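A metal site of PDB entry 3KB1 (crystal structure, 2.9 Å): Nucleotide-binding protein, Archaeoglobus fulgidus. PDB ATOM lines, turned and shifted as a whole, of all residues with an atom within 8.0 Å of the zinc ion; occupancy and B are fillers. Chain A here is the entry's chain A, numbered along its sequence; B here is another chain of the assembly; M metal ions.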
ATOM      1  N   PHE A 194      -7.940 -33.615 -10.390  1.00  0.00           N
ATOM      2  CA  PHE A 194      -8.241 -32.283 -10.878  1.00  0.00           C
ATOM      3  C   PHE A 194      -6.986 -31.434 -10.809  1.00  0.00           C
ATOM      4  O   PHE A 194      -6.249 -31.506  -9.834  1.00  0.00           O
ATOM      5  CB  PHE A 194      -9.325 -31.656  -9.985  1.00  0.00           C
ATOM      6  CG  PHE A 194      -9.832 -30.331 -10.496  1.00  0.00           C
ATOM      7  CD1 PHE A 194     -11.057 -30.261 -11.176  1.00  0.00           C
ATOM      8  CD2 PHE A 194      -9.104 -29.159 -10.308  1.00  0.00           C
ATOM      9  CE1 PHE A 194     -11.529 -29.037 -11.657  1.00  0.00           C
ATOM     10  CE2 PHE A 194      -9.576 -27.935 -10.788  1.00  0.00           C
ATOM     11  CZ  PHE A 194     -10.794 -27.873 -11.469  1.00  0.00           C
ATOM     12  N   GLU A 195      -6.737 -30.638 -11.845  1.00  0.00           N
ATOM     13  CA  GLU A 195      -5.562 -29.753 -11.828  1.00  0.00           C
ATOM     14  C   GLU A 195      -5.977 -28.298 -11.881  1.00  0.00           C
ATOM     15  O   GLU A 195      -6.572 -27.838 -12.849  1.00  0.00           O
ATOM     16  CB  GLU A 195      -4.627 -30.029 -12.996  1.00  0.00           C
ATOM     17  CG  GLU A 195      -3.743 -31.235 -12.865  1.00  0.00           C
ATOM     18  CD  GLU A 195      -2.520 -31.119 -13.758  1.00  0.00           C
ATOM     19  OE1 GLU A 195      -1.832 -32.149 -13.996  1.00  0.00           O
ATOM     20  OE2 GLU A 195      -2.250 -29.981 -14.228  1.00  0.00           O
ATOM     21  N   CYS A 196      -5.657 -27.555 -10.828  1.00  0.00           N
ATOM     22  CA  CYS A 196      -5.967 -26.144 -10.764  1.00  0.00           C
ATOM     23  C   CYS A 196      -5.052 -25.406 -11.760  1.00  0.00           C
ATOM     24  O   CYS A 196      -3.838 -25.415 -11.610  1.00  0.00           O
ATOM     25  CB  CYS A 196      -5.715 -25.635  -9.344  1.00  0.00           C
ATOM     26  SG  CYS A 196      -5.920 -23.870  -9.090  1.00  0.00           S
ATOM     27  N   PRO A 197      -5.642 -24.783 -12.790  1.00  0.00           N
ATOM     28  CA  PRO A 197      -4.879 -24.045 -13.816  1.00  0.00           C
ATOM     29  C   PRO A 197      -4.201 -22.788 -13.239  1.00  0.00           C
ATOM     30  O   PRO A 197      -3.391 -22.145 -13.910  1.00  0.00           O
ATOM     31  CB  PRO A 197      -5.949 -23.705 -14.851  1.00  0.00           C
ATOM     32  CG  PRO A 197      -7.157 -23.490 -13.997  1.00  0.00           C
ATOM     33  CD  PRO A 197      -7.092 -24.674 -13.053  1.00  0.00           C
ATOM     34  N   ASN A 198      -4.552 -22.470 -12.007  1.00  0.00           N
ATOM     35  CA  ASN A 198      -4.028 -21.307 -11.271  1.00  0.00           C
ATOM     36  C   ASN A 198      -2.623 -21.591 -10.729  1.00  0.00           C
ATOM     37  O   ASN A 198      -1.698 -20.800 -10.934  1.00  0.00           O
ATOM     38  CB  ASN A 198      -4.964 -20.967 -10.101  1.00  0.00           C
ATOM     39  CG  ASN A 198      -4.668 -19.604  -9.478  1.00  0.00           C
ATOM     40  OD1 ASN A 198      -4.948 -18.557 -10.066  1.00  0.00           O
ATOM     41  ND2 ASN A 198      -4.122 -19.620  -8.261  1.00  0.00           N
ATOM     42  N   CYS A 199      -2.471 -22.723 -10.037  1.00  0.00           N
ATOM     43  CA  CYS A 199      -1.185 -23.123  -9.457  1.00  0.00           C
ATOM     44  C   CYS A 199      -0.685 -24.484  -9.939  1.00  0.00           C
ATOM     45  O   CYS A 199       0.462 -24.856  -9.683  1.00  0.00           O
ATOM     46  CB  CYS A 199      -1.291 -23.164  -7.930  1.00  0.00           C
ATOM     47  SG  CYS A 199      -2.218 -24.583  -7.323  1.00  0.00           S
ATOM     48  N   GLY A 200      -1.534 -25.240 -10.635  1.00  0.00           N
ATOM     49  CA  GLY A 200      -1.112 -26.537 -11.132  1.00  0.00           C
ATOM     50  C   GLY A 200      -1.233 -27.671 -10.132  1.00  0.00           C
ATOM     51  O   GLY A 200      -0.804 -28.792 -10.388  1.00  0.00           O
ATOM     52  N   GLU A 201      -1.816 -27.368  -8.981  1.00  0.00           N
ATOM     53  CA  GLU A 201      -2.023 -28.365  -7.922  1.00  0.00           C
ATOM     54  C   GLU A 201      -2.878 -29.524  -8.433  1.00  0.00           C
ATOM     55  O   GLU A 201      -3.650 -29.376  -9.381  1.00  0.00           O
ATOM     56  CB  GLU A 201      -2.704 -27.684  -6.720  1.00  0.00           C
ATOM     57  CG  GLU A 201      -3.353 -28.600  -5.693  1.00  0.00           C
ATOM     58  CD  GLU A 201      -2.362 -29.509  -4.977  1.00  0.00           C
ATOM     59  OE1 GLU A 201      -2.803 -30.296  -4.113  1.00  0.00           O
ATOM     60  OE2 GLU A 201      -1.144 -29.429  -5.276  1.00  0.00           O
ATOM     61  N   ARG A 202      -2.730 -30.699  -7.822  1.00  0.00           N
ATOM     62  CA  ARG A 202      -3.521 -31.858  -8.207  1.00  0.00           C
ATOM     63  C   ARG A 202      -4.278 -32.407  -7.000  1.00  0.00           C
ATOM     64  O   ARG A 202      -3.683 -32.787  -5.996  1.00  0.00           O
ATOM     65  CB  ARG A 202      -2.627 -32.969  -8.782  1.00  0.00           C
ATOM     66  CG  ARG A 202      -2.769 -33.170 -10.258  1.00  0.00           C
ATOM     67  CD  ARG A 202      -1.425 -33.176 -10.931  1.00  0.00           C
ATOM     68  NE  ARG A 202      -1.275 -34.334 -11.799  1.00  0.00           N
ATOM     69  CZ  ARG A 202      -0.471 -34.381 -12.849  1.00  0.00           C
ATOM     70  NH1 ARG A 202      -0.400 -35.490 -13.579  1.00  0.00           N
ATOM     71  NH2 ARG A 202       0.263 -33.332 -13.180  1.00  0.00           N
ATOM     72  N   THR A 203      -5.595 -32.422  -7.072  1.00  0.00           N
ATOM     73  CA  THR A 203      -6.354 -32.959  -5.966  1.00  0.00           C
ATOM     74  C   THR A 203      -6.919 -34.278  -6.480  1.00  0.00           C
ATOM     75  O   THR A 203      -7.691 -34.289  -7.426  1.00  0.00           O
ATOM     76  CB  THR A 203      -7.488 -32.027  -5.546  1.00  0.00           C
ATOM     77  OG1 THR A 203      -6.944 -30.753  -5.169  1.00  0.00           O
ATOM     78  CG2 THR A 203      -8.242 -32.627  -4.378  1.00  0.00           C
ATOM     79  N   PHE B 194     -14.974 -26.190  -8.777  1.00  0.00           N
ATOM     80  CA  PHE B 194     -13.955 -26.902  -8.039  1.00  0.00           C
ATOM     81  C   PHE B 194     -13.073 -25.893  -7.322  1.00  0.00           C
ATOM     82  O   PHE B 194     -12.728 -24.860  -7.901  1.00  0.00           O
ATOM     83  CB  PHE B 194     -13.099 -27.712  -9.002  1.00  0.00           C
ATOM     84  CG  PHE B 194     -12.102 -28.627  -8.327  1.00  0.00           C
ATOM     85  CD1 PHE B 194     -12.373 -29.989  -8.188  1.00  0.00           C
ATOM     86  CD2 PHE B 194     -10.911 -28.130  -7.807  1.00  0.00           C
ATOM     87  CE1 PHE B 194     -11.473 -30.843  -7.542  1.00  0.00           C
ATOM     88  CE2 PHE B 194      -9.987 -28.977  -7.166  1.00  0.00           C
ATOM     89  CZ  PHE B 194     -10.273 -30.337  -7.029  1.00  0.00           C
ATOM     90  N   GLU B 195     -12.710 -26.173  -6.066  1.00  0.00           N
ATOM     91  CA  GLU B 195     -11.825 -25.267  -5.336  1.00  0.00           C
ATOM     92  C   GLU B 195     -10.520 -25.967  -4.964  1.00  0.00           C
ATOM     93  O   GLU B 195     -10.530 -26.936  -4.212  1.00  0.00           O
ATOM     94  CB  GLU B 195     -12.456 -24.742  -4.050  1.00  0.00           C
ATOM     95  CG  GLU B 195     -13.464 -23.629  -4.223  1.00  0.00           C
ATOM     96  CD  GLU B 195     -13.628 -22.831  -2.948  1.00  0.00           C
ATOM     97  OE1 GLU B 195     -14.613 -22.072  -2.830  1.00  0.00           O
ATOM     98  OE2 GLU B 195     -12.744 -22.974  -2.059  1.00  0.00           O
ATOM     99  N   CYS B 196      -9.424 -25.461  -5.489  1.00  0.00           N
ATOM    100  CA  CYS B 196      -8.113 -26.021  -5.203  1.00  0.00           C
ATOM    101  C   CYS B 196      -7.758 -25.662  -3.748  1.00  0.00           C
ATOM    102  O   CYS B 196      -7.634 -24.486  -3.412  1.00  0.00           O
ATOM    103  CB  CYS B 196      -7.086 -25.413  -6.158  1.00  0.00           C
ATOM    104  SG  CYS B 196      -5.379 -25.882  -5.859  1.00  0.00           S
ATOM    105  N   PRO B 197      -7.615 -26.672  -2.869  1.00  0.00           N
ATOM    106  CA  PRO B 197      -7.287 -26.454  -1.456  1.00  0.00           C
ATOM    107  C   PRO B 197      -5.862 -25.896  -1.272  1.00  0.00           C
ATOM    108  O   PRO B 197      -5.476 -25.506  -0.168  1.00  0.00           O
ATOM    109  CB  PRO B 197      -7.445 -27.855  -0.856  1.00  0.00           C
ATOM    110  CG  PRO B 197      -6.997 -28.726  -1.984  1.00  0.00           C
ATOM    111  CD  PRO B 197      -7.719 -28.109  -3.166  1.00  0.00           C
ATOM    112  N   ASN B 198      -5.108 -25.867  -2.369  1.00  0.00           N
ATOM    113  CA  ASN B 198      -3.729 -25.386  -2.406  1.00  0.00           C
ATOM    114  C   ASN B 198      -3.694 -23.847  -2.425  1.00  0.00           C
ATOM    115  O   ASN B 198      -2.983 -23.224  -1.637  1.00  0.00           O
ATOM    116  CB  ASN B 198      -3.026 -25.928  -3.660  1.00  0.00           C
ATOM    117  CG  ASN B 198      -1.510 -25.726  -3.638  1.00  0.00           C
ATOM    118  OD1 ASN B 198      -0.794 -26.397  -2.881  1.00  0.00           O
ATOM    119  ND2 ASN B 198      -1.021 -24.817  -4.470  1.00  0.00           N
ATOM    120  N   CYS B 199      -4.469 -23.252  -3.332  1.00  0.00           N
ATOM    121  CA  CYS B 199      -4.520 -21.799  -3.477  1.00  0.00           C
ATOM    122  C   CYS B 199      -5.934 -21.213  -3.313  1.00  0.00           C
ATOM    123  O   CYS B 199      -6.095 -20.004  -3.215  1.00  0.00           O
ATOM    124  CB  CYS B 199      -3.970 -21.375  -4.833  1.00  0.00           C
ATOM    125  SG  CYS B 199      -5.089 -21.722  -6.212  1.00  0.00           S
ATOM    126  N   GLY B 200      -6.944 -22.063  -3.301  1.00  0.00           N
ATOM    127  CA  GLY B 200      -8.309 -21.580  -3.145  1.00  0.00           C
ATOM    128  C   GLY B 200      -8.969 -21.133  -4.429  1.00  0.00           C
ATOM    129  O   GLY B 200     -10.085 -20.605  -4.422  1.00  0.00           O
ATOM    130  N   GLU B 201      -8.284 -21.349  -5.544  1.00  0.00           N
ATOM    131  CA  GLU B 201      -8.807 -20.981  -6.867  1.00  0.00           C
ATOM    132  C   GLU B 201     -10.127 -21.700  -7.143  1.00  0.00           C
ATOM    133  O   GLU B 201     -10.401 -22.763  -6.576  1.00  0.00           O
ATOM    134  CB  GLU B 201      -7.763 -21.350  -7.927  1.00  0.00           C
ATOM    135  CG  GLU B 201      -8.251 -21.414  -9.376  1.00  0.00           C
ATOM    136  CD  GLU B 201      -8.745 -20.077  -9.912  1.00  0.00           C
ATOM    137  OE1 GLU B 201      -9.166 -20.033 -11.088  1.00  0.00           O
ATOM    138  OE2 GLU B 201      -8.709 -19.074  -9.149  1.00  0.00           O
ATOM    139  N   ARG B 202     -10.956 -21.126  -8.002  1.00  0.00           N
ATOM    140  CA  ARG B 202     -12.221 -21.742  -8.372  1.00  0.00           C
ATOM    141  C   ARG B 202     -12.311 -21.924  -9.886  1.00  0.00           C
ATOM    142  O   ARG B 202     -12.234 -20.964 -10.646  1.00  0.00           O
ATOM    143  CB  ARG B 202     -13.407 -20.883  -7.903  1.00  0.00           C
ATOM    144  CG  ARG B 202     -14.168 -21.475  -6.735  1.00  0.00           C
ATOM    145  CD  ARG B 202     -14.358 -20.459  -5.642  1.00  0.00           C
ATOM    146  NE  ARG B 202     -15.747 -20.370  -5.232  1.00  0.00           N
ATOM    147  CZ  ARG B 202     -16.148 -19.963  -4.035  1.00  0.00           C
ATOM    148  NH1 ARG B 202     -17.446 -19.913  -3.749  1.00  0.00           N
ATOM    149  NH2 ARG B 202     -15.264 -19.629  -3.111  1.00  0.00           N
ATOM    150  N   THR B 203     -12.440 -23.156 -10.337  1.00  0.00           N
ATOM    151  CA  THR B 203     -12.557 -23.376 -11.760  1.00  0.00           C
ATOM    152  C   THR B 203     -14.001 -23.792 -11.963  1.00  0.00           C
ATOM    153  O   THR B 203     -14.429 -24.817 -11.440  1.00  0.00           O
ATOM    154  CB  THR B 203     -11.613 -24.472 -12.249  1.00  0.00           C
ATOM    155  OG1 THR B 203     -10.258 -24.108 -11.939  1.00  0.00           O
ATOM    156  CG2 THR B 203     -11.757 -24.661 -13.744  1.00  0.00           C
HETATM  157 ZN    ZN M   1      -4.656 -24.024  -7.142  1.00  0.00          ZN
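The zinc ion is bound by the side-chain sulfur (SG) of Cys 196 of chain A (2.3 Å). The zinc ion is bound by SG of Cys 196 of chain B, at 2.4 Å. SG of Cys 199 of chain A is bound to the zinc ion, 2.5 Å away. The side-chain sulfur (SG) of Cys 199 of chain B is bound to the zinc ion (2.5 Å).
Of the 20 residues printed, 4 come within 4 Å of the zinc ion.
SG of Cys 199 of chain A sits close to N of Glu 201 of chain A, 3.3 Å away. SG of Cys 199 of chain B lies close to ND2 of Asn 198 of chain A (3.1 Å). SG of Cys 196 of chain A sits close to N of Asn 198 of chain A. The backbone NH (N) of Cys 196 of chain A lies within hydrogen-bond range of the backbone carbonyl oxygen (O) of Glu 201 of chain A, 3.1 Å away. SG of Cys 199 of chain B sits close to N of Glu 201 of chain B, at 3.3 Å. ND2 of Asn 198 of chain B lies close to SG of Cys 199 of chain A (3.1 Å). N of Asn 198 of chain B lies close to SG of Cys 196 of chain B (3.5 Å). N of Cys 196 of chain B is in hydrogen-bond range of O of Glu 201 of chain B, at 3.1 Å.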
